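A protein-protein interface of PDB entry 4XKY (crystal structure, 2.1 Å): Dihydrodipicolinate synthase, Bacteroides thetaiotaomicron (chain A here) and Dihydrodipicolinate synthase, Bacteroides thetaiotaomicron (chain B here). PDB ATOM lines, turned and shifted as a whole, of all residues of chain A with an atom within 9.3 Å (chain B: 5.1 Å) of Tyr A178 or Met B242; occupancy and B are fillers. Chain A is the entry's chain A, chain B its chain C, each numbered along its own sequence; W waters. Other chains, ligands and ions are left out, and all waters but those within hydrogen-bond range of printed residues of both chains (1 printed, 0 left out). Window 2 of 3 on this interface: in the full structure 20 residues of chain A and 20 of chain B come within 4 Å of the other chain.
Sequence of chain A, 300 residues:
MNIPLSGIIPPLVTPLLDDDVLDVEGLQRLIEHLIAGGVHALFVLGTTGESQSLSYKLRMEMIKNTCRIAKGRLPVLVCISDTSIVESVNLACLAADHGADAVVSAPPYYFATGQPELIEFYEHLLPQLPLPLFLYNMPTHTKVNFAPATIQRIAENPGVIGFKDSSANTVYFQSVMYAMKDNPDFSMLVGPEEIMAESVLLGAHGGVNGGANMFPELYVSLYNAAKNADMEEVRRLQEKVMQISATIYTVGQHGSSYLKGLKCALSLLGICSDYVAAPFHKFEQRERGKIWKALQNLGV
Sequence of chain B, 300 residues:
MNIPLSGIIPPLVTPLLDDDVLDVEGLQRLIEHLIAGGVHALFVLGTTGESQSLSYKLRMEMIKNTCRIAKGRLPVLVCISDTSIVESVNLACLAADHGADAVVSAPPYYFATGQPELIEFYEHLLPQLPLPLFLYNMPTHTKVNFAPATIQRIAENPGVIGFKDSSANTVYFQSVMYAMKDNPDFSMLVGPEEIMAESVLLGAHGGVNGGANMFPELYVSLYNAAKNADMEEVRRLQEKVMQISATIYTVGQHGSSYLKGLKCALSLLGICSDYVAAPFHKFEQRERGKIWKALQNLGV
The side-chain amide oxygen (OE1) of Gln A174 sits close to the side-chain amide oxygen (OE1) of Gln B238, at 3.4 Å.
O of Val A171 is in hydrogen-bond range of OG of Ser A175 (3.0 Å).
The side-chain carboxylate of Glu B194 sits at hydrogen-bond distance from the side-chain hydroxyl of Ser B245 (2.6 Å).
The side-chain amide oxygen (OE1) of Gln B238 sits close to the backbone carbonyl oxygen (O) of Glu B194 (3.0 Å).
The side-chain amide oxygen of Gln B238 sits close to the side-chain sulfur of Met B242 (3.5 Å).
The backbone carbonyl oxygen (O) of Gln B243 sits at hydrogen-bond distance from the side-chain hydroxyl (OG1) of Thr B247 (2.7 Å).
Glu B194 touches Val A171.
Gln A174 touches Glu B194 (CG to O, 3.8 Å).
Gln A174 touches Met B242 (C to CE, 3.6 Å).
N of Ser A175 touches CE of Met B242 (3.6 Å).
O of Glu B239 touches CE1 of Tyr A178, 3.7 Å away.
CD1 of Tyr A178 touches CB of Met B242, 3.5 Å away.
Tyr A178 touches Gln B243.
Tyr A178 touches three residues of chain B.
Printed residues of chain A within 4 Å of Met B242: Gln A174, Ser A175 and Tyr A178.
Of the printed residues of chain A, Glu B194 touches Val A171 and Gln A174.
Printed residues of chain A within 4 Å of Gln B238: Gln A174 (3.4 Å).
Of the printed residues of chain A, Glu B239 touches Tyr A178 (3.7 Å).
Of the printed residues of chain B, Gln A174 touches Glu B194 (3.8 Å), Gln B238 (3.4 Å) and Met B242 (3.6 Å).
Thr B247 touches none of the printed residues of chain A.
Tyr A172 touches none of the printed residues of chain B.
Printed residues of chain A that touch a printed residue of chain B: Val A171, Gln A174, Ser A175 and Tyr A178.
Hydrophobic or aromatic side chains of chain A within 4 Å of the printed part of chain B: Val A171 and Tyr A178.
Of the 11 printed residues of chain B, 5 touch a printed residue of chain A.
Hydrophobic or aromatic side chains of chain B within 4 Å of the printed part of chain A: Met B242.
Water W1 lies within hydrogen-bond range of OG of Ser B245 and OG of Ser A175.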
ATOM      1  N   PRO A 148     -15.256 -20.892 -14.001  1.00  0.00           N
ATOM      2  CA  PRO A 148     -13.970 -21.544 -13.781  1.00  0.00           C
ATOM      3  C   PRO A 148     -14.078 -23.032 -13.502  1.00  0.00           C
ATOM      4  O   PRO A 148     -13.381 -23.813 -14.143  1.00  0.00           O
ATOM      5  CB  PRO A 148     -13.421 -20.799 -12.575  1.00  0.00           C
ATOM      6  CG  PRO A 148     -13.894 -19.410 -12.802  1.00  0.00           C
ATOM      7  CD  PRO A 148     -15.297 -19.573 -13.341  1.00  0.00           C
ATOM      8  N   ALA A 149     -14.955 -23.417 -12.574  1.00  0.00           N
ATOM      9  CA  ALA A 149     -15.104 -24.823 -12.209  1.00  0.00           C
ATOM     10  C   ALA A 149     -15.568 -25.650 -13.418  1.00  0.00           C
ATOM     11  O   ALA A 149     -15.160 -26.789 -13.568  1.00  0.00           O
ATOM     12  CB  ALA A 149     -16.063 -24.985 -11.033  1.00  0.00           C
ATOM     13  N   ILE A 151     -14.793 -25.098 -16.571  1.00  0.00           N
ATOM     14  CA  ILE A 151     -13.612 -25.329 -17.386  1.00  0.00           C
ATOM     15  C   ILE A 151     -12.739 -26.417 -16.784  1.00  0.00           C
ATOM     16  O   ILE A 151     -12.254 -27.276 -17.516  1.00  0.00           O
ATOM     17  CB  ILE A 151     -12.815 -24.033 -17.623  1.00  0.00           C
ATOM     18  CG1 ILE A 151     -13.527 -23.204 -18.686  1.00  0.00           C
ATOM     19  CG2 ILE A 151     -11.416 -24.316 -18.133  1.00  0.00           C
ATOM     20  CD1 ILE A 151     -13.103 -21.753 -18.705  1.00  0.00           C
ATOM     21  N   GLN A 152     -12.534 -26.384 -15.468  1.00  0.00           N
ATOM     22  CA  GLN A 152     -11.816 -27.468 -14.772  1.00  0.00           C
ATOM     23  C   GLN A 152     -12.407 -28.802 -15.135  1.00  0.00           C
ATOM     24  O   GLN A 152     -11.697 -29.740 -15.492  1.00  0.00           O
ATOM     25  CB  GLN A 152     -11.949 -27.354 -13.258  1.00  0.00           C
ATOM     26  CG  GLN A 152     -10.718 -26.904 -12.503  1.00  0.00           C
ATOM     27  CD  GLN A 152     -11.012 -26.758 -11.019  1.00  0.00           C
ATOM     28  OE1 GLN A 152     -10.727 -25.723 -10.408  1.00  0.00           O
ATOM     29  NE2 GLN A 152     -11.604 -27.796 -10.432  1.00  0.00           N
ATOM     30  N   THR A 170     -10.257  -9.413 -17.844  1.00  0.00           N
ATOM     31  CA  THR A 170      -9.096 -10.088 -17.278  1.00  0.00           C
ATOM     32  C   THR A 170      -9.254 -10.525 -15.835  1.00  0.00           C
ATOM     33  O   THR A 170      -8.469 -11.333 -15.362  1.00  0.00           O
ATOM     34  CB  THR A 170      -7.799  -9.257 -17.440  1.00  0.00           C
ATOM     35  OG1 THR A 170      -8.121  -7.866 -17.363  1.00  0.00           O
ATOM     36  CG2 THR A 170      -7.163  -9.554 -18.784  1.00  0.00           C
ATOM     37  N   VAL A 171     -10.266 -10.024 -15.142  1.00  0.00           N
ATOM     38  CA  VAL A 171     -10.642 -10.588 -13.851  1.00  0.00           C
ATOM     39  C   VAL A 171     -11.087 -12.027 -14.093  1.00  0.00           C
ATOM     40  O   VAL A 171     -10.646 -12.964 -13.426  1.00  0.00           O
ATOM     41  CB  VAL A 171     -11.814  -9.821 -13.214  1.00  0.00           C
ATOM     42  CG1 VAL A 171     -12.379 -10.571 -12.005  1.00  0.00           C
ATOM     43  CG2 VAL A 171     -11.355  -8.433 -12.809  1.00  0.00           C
ATOM     44  N   TYR A 172     -11.983 -12.176 -15.063  1.00  0.00           N
ATOM     45  CA  TYR A 172     -12.498 -13.497 -15.448  1.00  0.00           C
ATOM     46  C   TYR A 172     -11.360 -14.392 -15.931  1.00  0.00           C
ATOM     47  O   TYR A 172     -11.247 -15.529 -15.495  1.00  0.00           O
ATOM     48  CB  TYR A 172     -13.589 -13.382 -16.514  1.00  0.00           C
ATOM     49  CG  TYR A 172     -13.938 -14.704 -17.159  1.00  0.00           C
ATOM     50  CD1 TYR A 172     -14.764 -15.610 -16.507  1.00  0.00           C
ATOM     51  CD2 TYR A 172     -13.423 -15.059 -18.410  1.00  0.00           C
ATOM     52  CE1 TYR A 172     -15.090 -16.822 -17.080  1.00  0.00           C
ATOM     53  CE2 TYR A 172     -13.761 -16.277 -19.003  1.00  0.00           C
ATOM     54  CZ  TYR A 172     -14.587 -17.154 -18.330  1.00  0.00           C
ATOM     55  OH  TYR A 172     -14.916 -18.377 -18.885  1.00  0.00           O
ATOM     56  N   PHE A 173     -10.488 -13.876 -16.784  1.00  0.00           N
ATOM     57  CA  PHE A 173      -9.391 -14.705 -17.288  1.00  0.00           C
ATOM     58  C   PHE A 173      -8.466 -15.215 -16.174  1.00  0.00           C
ATOM     59  O   PHE A 173      -8.033 -16.359 -16.214  1.00  0.00           O
ATOM     60  CB  PHE A 173      -8.554 -13.982 -18.335  1.00  0.00           C
ATOM     61  CG  PHE A 173      -7.585 -14.890 -19.054  1.00  0.00           C
ATOM     62  CD1 PHE A 173      -8.010 -15.688 -20.110  1.00  0.00           C
ATOM     63  CD2 PHE A 173      -6.262 -14.989 -18.642  1.00  0.00           C
ATOM     64  CE1 PHE A 173      -7.116 -16.528 -20.779  1.00  0.00           C
ATOM     65  CE2 PHE A 173      -5.371 -15.831 -19.292  1.00  0.00           C
ATOM     66  CZ  PHE A 173      -5.800 -16.613 -20.359  1.00  0.00           C
ATOM     67  N   GLN A 174      -8.137 -14.349 -15.218  1.00  0.00           N
ATOM     68  CA  GLN A 174      -7.286 -14.701 -14.077  1.00  0.00           C
ATOM     69  C   GLN A 174      -8.004 -15.727 -13.181  1.00  0.00           C
ATOM     70  O   GLN A 174      -7.358 -16.626 -12.638  1.00  0.00           O
ATOM     71  CB  GLN A 174      -6.916 -13.450 -13.268  1.00  0.00           C
ATOM     72  CG  GLN A 174      -5.924 -12.519 -13.947  1.00  0.00           C
ATOM     73  CD  GLN A 174      -4.600 -13.212 -14.184  1.00  0.00           C
ATOM     74  OE1 GLN A 174      -4.062 -13.832 -13.279  1.00  0.00           O
ATOM     75  NE2 GLN A 174      -4.084 -13.129 -15.400  1.00  0.00           N
ATOM     76  N   SER A 175      -9.331 -15.607 -13.041  1.00  0.00           N
ATOM     77  CA  SER A 175     -10.088 -16.618 -12.292  1.00  0.00           C
ATOM     78  C   SER A 175      -9.934 -18.016 -12.910  1.00  0.00           C
ATOM     79  O   SER A 175      -9.871 -19.003 -12.183  1.00  0.00           O
ATOM     80  CB  SER A 175     -11.575 -16.272 -12.187  1.00  0.00           C
ATOM     81  OG  SER A 175     -11.760 -15.034 -11.532  1.00  0.00           O
ATOM     82  N   VAL A 176      -9.887 -18.089 -14.242  1.00  0.00           N
ATOM     83  CA  VAL A 176      -9.760 -19.376 -14.937  1.00  0.00           C
ATOM     84  C   VAL A 176      -8.304 -19.854 -14.845  1.00  0.00           C
ATOM     85  O   VAL A 176      -8.081 -21.033 -14.572  1.00  0.00           O
ATOM     86  CB  VAL A 176     -10.242 -19.312 -16.407  1.00  0.00           C
ATOM     87  CG1 VAL A 176     -10.173 -20.674 -17.075  1.00  0.00           C
ATOM     88  CG2 VAL A 176     -11.673 -18.800 -16.495  1.00  0.00           C
ATOM     89  N   MET A 177      -7.322 -18.960 -15.047  1.00  0.00           N
ATOM     90  CA  MET A 177      -5.913 -19.312 -14.756  1.00  0.00           C
ATOM     91  C   MET A 177      -5.802 -19.974 -13.369  1.00  0.00           C
ATOM     92  O   MET A 177      -5.232 -21.068 -13.217  1.00  0.00           O
ATOM     93  CB  MET A 177      -4.988 -18.085 -14.805  1.00  0.00           C
ATOM     94  CG  MET A 177      -4.779 -17.505 -16.197  1.00  0.00           C
ATOM     95  SD  MET A 177      -3.743 -18.538 -17.268  1.00  0.00           S
ATOM     96  CE  MET A 177      -2.162 -18.371 -16.437  1.00  0.00           C
ATOM     97  N   TYR A 178      -6.383 -19.332 -12.360  1.00  0.00           N
ATOM     98  CA  TYR A 178      -6.248 -19.839 -11.003  1.00  0.00           C
ATOM     99  C   TYR A 178      -6.876 -21.225 -10.891  1.00  0.00           C
ATOM    100  O   TYR A 178      -6.273 -22.109 -10.318  1.00  0.00           O
ATOM    101  CB  TYR A 178      -6.851 -18.889  -9.984  1.00  0.00           C
ATOM    102  CG  TYR A 178      -6.833 -19.426  -8.569  1.00  0.00           C
ATOM    103  CD1 TYR A 178      -5.765 -19.162  -7.727  1.00  0.00           C
ATOM    104  CD2 TYR A 178      -7.888 -20.180  -8.067  1.00  0.00           C
ATOM    105  CE1 TYR A 178      -5.733 -19.648  -6.427  1.00  0.00           C
ATOM    106  CE2 TYR A 178      -7.864 -20.663  -6.764  1.00  0.00           C
ATOM    107  CZ  TYR A 178      -6.777 -20.384  -5.958  1.00  0.00           C
ATOM    108  OH  TYR A 178      -6.697 -20.826  -4.669  1.00  0.00           O
ATOM    109  N   ALA A 179      -8.073 -21.394 -11.449  1.00  0.00           N
ATOM    110  CA  ALA A 179      -8.748 -22.698 -11.488  1.00  0.00           C
ATOM    111  C   ALA A 179      -7.956 -23.774 -12.254  1.00  0.00           C
ATOM    112  O   ALA A 179      -8.089 -24.959 -11.954  1.00  0.00           O
ATOM    113  CB  ALA A 179     -10.151 -22.559 -12.081  1.00  0.00           C
ATOM    114  N   MET A 180      -7.137 -23.370 -13.227  1.00  0.00           N
ATOM    115  CA  MET A 180      -6.382 -24.331 -14.047  1.00  0.00           C
ATOM    116  C   MET A 180      -4.899 -24.443 -13.681  1.00  0.00           C
ATOM    117  O   MET A 180      -4.127 -25.087 -14.395  1.00  0.00           O
ATOM    118  CB  MET A 180      -6.510 -23.959 -15.537  1.00  0.00           C
ATOM    119  CG  MET A 180      -7.940 -23.961 -16.051  1.00  0.00           C
ATOM    120  SD  MET A 180      -8.752 -25.538 -15.750  1.00  0.00           S
ATOM    121  CE  MET A 180      -7.814 -26.672 -16.772  1.00  0.00           C
ATOM    122  N   LYS A 181      -4.508 -23.844 -12.562  1.00  0.00           N
ATOM    123  CA  LYS A 181      -3.090 -23.713 -12.211  1.00  0.00           C
ATOM    124  C   LYS A 181      -2.375 -25.040 -11.961  1.00  0.00           C
ATOM    125  O   LYS A 181      -1.163 -25.097 -12.055  1.00  0.00           O
ATOM    126  CB  LYS A 181      -2.937 -22.852 -10.968  1.00  0.00           C
ATOM    127  CG  LYS A 181      -3.468 -23.521  -9.705  1.00  0.00           C
ATOM    128  CD  LYS A 181      -3.325 -22.580  -8.533  1.00  0.00           C
ATOM    129  CE  LYS A 181      -4.286 -22.950  -7.431  1.00  0.00           C
ATOM    130  NZ  LYS A 181      -3.669 -24.019  -6.617  1.00  0.00           N
ATOM    131  N   ASP A 182      -3.121 -26.089 -11.621  1.00  0.00           N
ATOM    132  CA  ASP A 182      -2.526 -27.417 -11.428  1.00  0.00           C
ATOM    133  C   ASP A 182      -2.575 -28.316 -12.665  1.00  0.00           C
ATOM    134  O   ASP A 182      -2.305 -29.513 -12.575  1.00  0.00           O
ATOM    135  CB  ASP A 182      -3.180 -28.113 -10.236  1.00  0.00           C
ATOM    136  CG  ASP A 182      -2.842 -27.437  -8.922  1.00  0.00           C
ATOM    137  OD1 ASP A 182      -1.716 -26.909  -8.787  1.00  0.00           O
ATOM    138  OD2 ASP A 182      -3.704 -27.433  -8.027  1.00  0.00           O
ATOM    139  N   ASN A 183      -2.901 -27.738 -13.816  1.00  0.00           N
ATOM    140  CA  ASN A 183      -2.873 -28.462 -15.072  1.00  0.00           C
ATOM    141  C   ASN A 183      -2.090 -27.645 -16.091  1.00  0.00           C
ATOM    142  O   ASN A 183      -2.666 -27.104 -17.039  1.00  0.00           O
ATOM    143  CB  ASN A 183      -4.293 -28.734 -15.560  1.00  0.00           C
ATOM    144  CG  ASN A 183      -4.340 -29.775 -16.665  1.00  0.00           C
ATOM    145  OD1 ASN A 183      -3.307 -30.293 -17.116  1.00  0.00           O
ATOM    146  ND2 ASN A 183      -5.548 -30.100 -17.097  1.00  0.00           N
ATOM    147  N   MET A 188      -3.825 -22.050 -22.272  1.00  0.00           N
ATOM    148  CA  MET A 188      -4.648 -20.885 -21.923  1.00  0.00           C
ATOM    149  C   MET A 188      -4.248 -19.702 -22.816  1.00  0.00           C
ATOM    150  O   MET A 188      -3.147 -19.143 -22.669  1.00  0.00           O
ATOM    151  CB  MET A 188      -4.475 -20.491 -20.452  1.00  0.00           C
ATOM    152  CG  MET A 188      -4.982 -21.508 -19.427  1.00  0.00           C
ATOM    153  SD  MET A 188      -6.780 -21.516 -19.359  1.00  0.00           S
ATOM    154  CE  MET A 188      -7.043 -19.933 -18.566  1.00  0.00           C
ATOM    155  N   LEU A 202       1.868 -12.793 -16.768  1.00  0.00           N
ATOM    156  CA  LEU A 202       1.305 -13.571 -15.675  1.00  0.00           C
ATOM    157  C   LEU A 202       0.988 -15.002 -16.085  1.00  0.00           C
ATOM    158  O   LEU A 202       0.110 -15.625 -15.509  1.00  0.00           O
ATOM    159  CB  LEU A 202       0.022 -12.903 -15.185  1.00  0.00           C
ATOM    160  CG  LEU A 202       0.204 -11.920 -14.050  1.00  0.00           C
ATOM    161  CD1 LEU A 202       1.046 -10.730 -14.461  1.00  0.00           C
ATOM    162  CD2 LEU A 202      -1.174 -11.467 -13.599  1.00  0.00           C
ATOM    163  N   GLU B 194      -8.019  -8.413  -8.768  1.00  0.00           N
ATOM    164  CA  GLU B 194      -7.503  -9.554  -9.531  1.00  0.00           C
ATOM    165  C   GLU B 194      -6.607  -9.132 -10.711  1.00  0.00           C
ATOM    166  O   GLU B 194      -5.789  -9.927 -11.186  1.00  0.00           O
ATOM    167  CB  GLU B 194      -8.679 -10.396 -10.063  1.00  0.00           C
ATOM    168  CG  GLU B 194      -9.560 -11.037  -8.980  1.00  0.00           C
ATOM    169  CD  GLU B 194     -10.707 -10.150  -8.487  1.00  0.00           C
ATOM    170  OE1 GLU B 194     -10.822  -8.978  -8.931  1.00  0.00           O
ATOM    171  OE2 GLU B 194     -11.516 -10.639  -7.662  1.00  0.00           O
ATOM    172  N   GLN B 238       0.222 -12.854  -6.338  1.00  0.00           N
ATOM    173  CA  GLN B 238      -0.987 -12.963  -7.155  1.00  0.00           C
ATOM    174  C   GLN B 238      -1.808 -14.212  -6.822  1.00  0.00           C
ATOM    175  O   GLN B 238      -3.036 -14.137  -6.745  1.00  0.00           O
ATOM    176  CB  GLN B 238      -0.664 -12.926  -8.646  1.00  0.00           C
ATOM    177  CG  GLN B 238      -1.847 -13.132  -9.579  1.00  0.00           C
ATOM    178  CD  GLN B 238      -2.828 -11.971  -9.653  1.00  0.00           C
ATOM    179  OE1 GLN B 238      -3.813 -12.053 -10.396  1.00  0.00           O
ATOM    180  NE2 GLN B 238      -2.579 -10.891  -8.911  1.00  0.00           N
ATOM    181  N   GLU B 239      -1.149 -15.346  -6.606  1.00  0.00           N
ATOM    182  CA  GLU B 239      -1.879 -16.553  -6.249  1.00  0.00           C
ATOM    183  C   GLU B 239      -2.659 -16.410  -4.920  1.00  0.00           C
ATOM    184  O   GLU B 239      -3.702 -17.027  -4.735  1.00  0.00           O
ATOM    185  CB  GLU B 239      -0.947 -17.747  -6.190  1.00  0.00           C
ATOM    186  CG  GLU B 239      -1.654 -19.031  -5.773  1.00  0.00           C
ATOM    187  CD  GLU B 239      -0.785 -20.262  -5.914  1.00  0.00           C
ATOM    188  OE1 GLU B 239      -0.108 -20.405  -6.954  1.00  0.00           O
ATOM    189  OE2 GLU B 239      -0.799 -21.098  -4.989  1.00  0.00           O
ATOM    190  N   LYS B 240      -2.154 -15.607  -3.997  1.00  0.00           N
ATOM    191  CA  LYS B 240      -2.875 -15.354  -2.765  1.00  0.00           C
ATOM    192  C   LYS B 240      -4.109 -14.480  -2.982  1.00  0.00           C
ATOM    193  O   LYS B 240      -5.174 -14.755  -2.419  1.00  0.00           O
ATOM    194  CB  LYS B 240      -1.956 -14.714  -1.743  1.00  0.00           C
ATOM    195  CG  LYS B 240      -0.877 -15.646  -1.199  1.00  0.00           C
ATOM    196  CD  LYS B 240      -0.313 -15.070   0.091  1.00  0.00           C
ATOM    197  CE  LYS B 240       1.119 -15.497   0.372  1.00  0.00           C
ATOM    198  NZ  LYS B 240       1.216 -16.877   0.916  1.00  0.00           N
ATOM    199  N   VAL B 241      -3.962 -13.437  -3.802  1.00  0.00           N
ATOM    200  CA  VAL B 241      -5.060 -12.540  -4.112  1.00  0.00           C
ATOM    201  C   VAL B 241      -6.121 -13.374  -4.816  1.00  0.00           C
ATOM    202  O   VAL B 241      -7.303 -13.263  -4.524  1.00  0.00           O
ATOM    203  CB  VAL B 241      -4.595 -11.363  -4.994  1.00  0.00           C
ATOM    204  CG1 VAL B 241      -5.767 -10.638  -5.616  1.00  0.00           C
ATOM    205  CG2 VAL B 241      -3.744 -10.387  -4.193  1.00  0.00           C
ATOM    206  N   MET B 242      -5.696 -14.257  -5.711  1.00  0.00           N
ATOM    207  CA  MET B 242      -6.673 -15.057  -6.444  1.00  0.00           C
ATOM    208  C   MET B 242      -7.383 -16.091  -5.548  1.00  0.00           C
ATOM    209  O   MET B 242      -8.569 -16.365  -5.744  1.00  0.00           O
ATOM    210  CB  MET B 242      -6.039 -15.707  -7.688  1.00  0.00           C
ATOM    211  CG  MET B 242      -5.633 -14.715  -8.786  1.00  0.00           C
ATOM    212  SD  MET B 242      -6.814 -13.387  -9.180  1.00  0.00           S
ATOM    213  CE  MET B 242      -8.125 -14.416  -9.832  1.00  0.00           C
ATOM    214  N   GLN B 243      -6.676 -16.656  -4.573  1.00  0.00           N
ATOM    215  CA  GLN B 243      -7.313 -17.583  -3.631  1.00  0.00           C
ATOM    216  C   GLN B 243      -8.399 -16.884  -2.814  1.00  0.00           C
ATOM    217  O   GLN B 243      -9.493 -17.410  -2.631  1.00  0.00           O
ATOM    218  CB  GLN B 243      -6.287 -18.220  -2.690  1.00  0.00           C
ATOM    219  CG  GLN B 243      -6.921 -19.273  -1.785  1.00  0.00           C
ATOM    220  CD  GLN B 243      -5.950 -19.930  -0.831  1.00  0.00           C
ATOM    221  OE1 GLN B 243      -4.796 -19.526  -0.720  1.00  0.00           O
ATOM    222  NE2 GLN B 243      -6.434 -20.936  -0.099  1.00  0.00           N
ATOM    223  N   ILE B 244      -8.067 -15.700  -2.317  1.00  0.00           N
ATOM    224  CA  ILE B 244      -9.026 -14.819  -1.672  1.00  0.00           C
ATOM    225  C   ILE B 244     -10.245 -14.588  -2.555  1.00  0.00           C
ATOM    226  O   ILE B 244     -11.382 -14.669  -2.077  1.00  0.00           O
ATOM    227  CB  ILE B 244      -8.376 -13.450  -1.347  1.00  0.00           C
ATOM    228  CG1 ILE B 244      -7.474 -13.563  -0.118  1.00  0.00           C
ATOM    229  CG2 ILE B 244      -9.416 -12.366  -1.101  1.00  0.00           C
ATOM    230  CD1 ILE B 244      -6.336 -12.560  -0.088  1.00  0.00           C
ATOM    231  N   SER B 245     -10.009 -14.263  -3.824  1.00  0.00           N
ATOM    232  CA  SER B 245     -11.093 -13.921  -4.751  1.00  0.00           C
ATOM    233  C   SER B 245     -12.031 -15.107  -4.930  1.00  0.00           C
ATOM    234  O   SER B 245     -13.266 -14.963  -4.881  1.00  0.00           O
ATOM    235  CB  SER B 245     -10.551 -13.478  -6.128  1.00  0.00           C
ATOM    236  OG  SER B 245     -11.607 -13.217  -7.068  1.00  0.00           O
ATOM    237  N   ALA B 246     -11.428 -16.270  -5.141  1.00  0.00           N
ATOM    238  CA  ALA B 246     -12.164 -17.513  -5.337  1.00  0.00           C
ATOM    239  C   ALA B 246     -12.857 -18.039  -4.061  1.00  0.00           C
ATOM    240  O   ALA B 246     -13.825 -18.802  -4.170  1.00  0.00           O
ATOM    241  CB  ALA B 246     -11.228 -18.580  -5.890  1.00  0.00           C
ATOM    242  N   THR B 247     -12.375 -17.656  -2.866  1.00  0.00           N
ATOM    243  CA  THR B 247     -12.843 -18.302  -1.611  1.00  0.00           C
ATOM    244  C   THR B 247     -13.599 -17.376  -0.638  1.00  0.00           C
ATOM    245  O   THR B 247     -14.534 -17.821   0.024  1.00  0.00           O
ATOM    246  CB  THR B 247     -11.726 -19.074  -0.843  1.00  0.00           C
ATOM    247  OG1 THR B 247     -10.724 -18.178  -0.351  1.00  0.00           O
ATOM    248  CG2 THR B 247     -11.068 -20.204  -1.701  1.00  0.00           C
HETATM  249  O   HOH W   1     -11.785 -15.377  -8.675  1.00  0.00           O
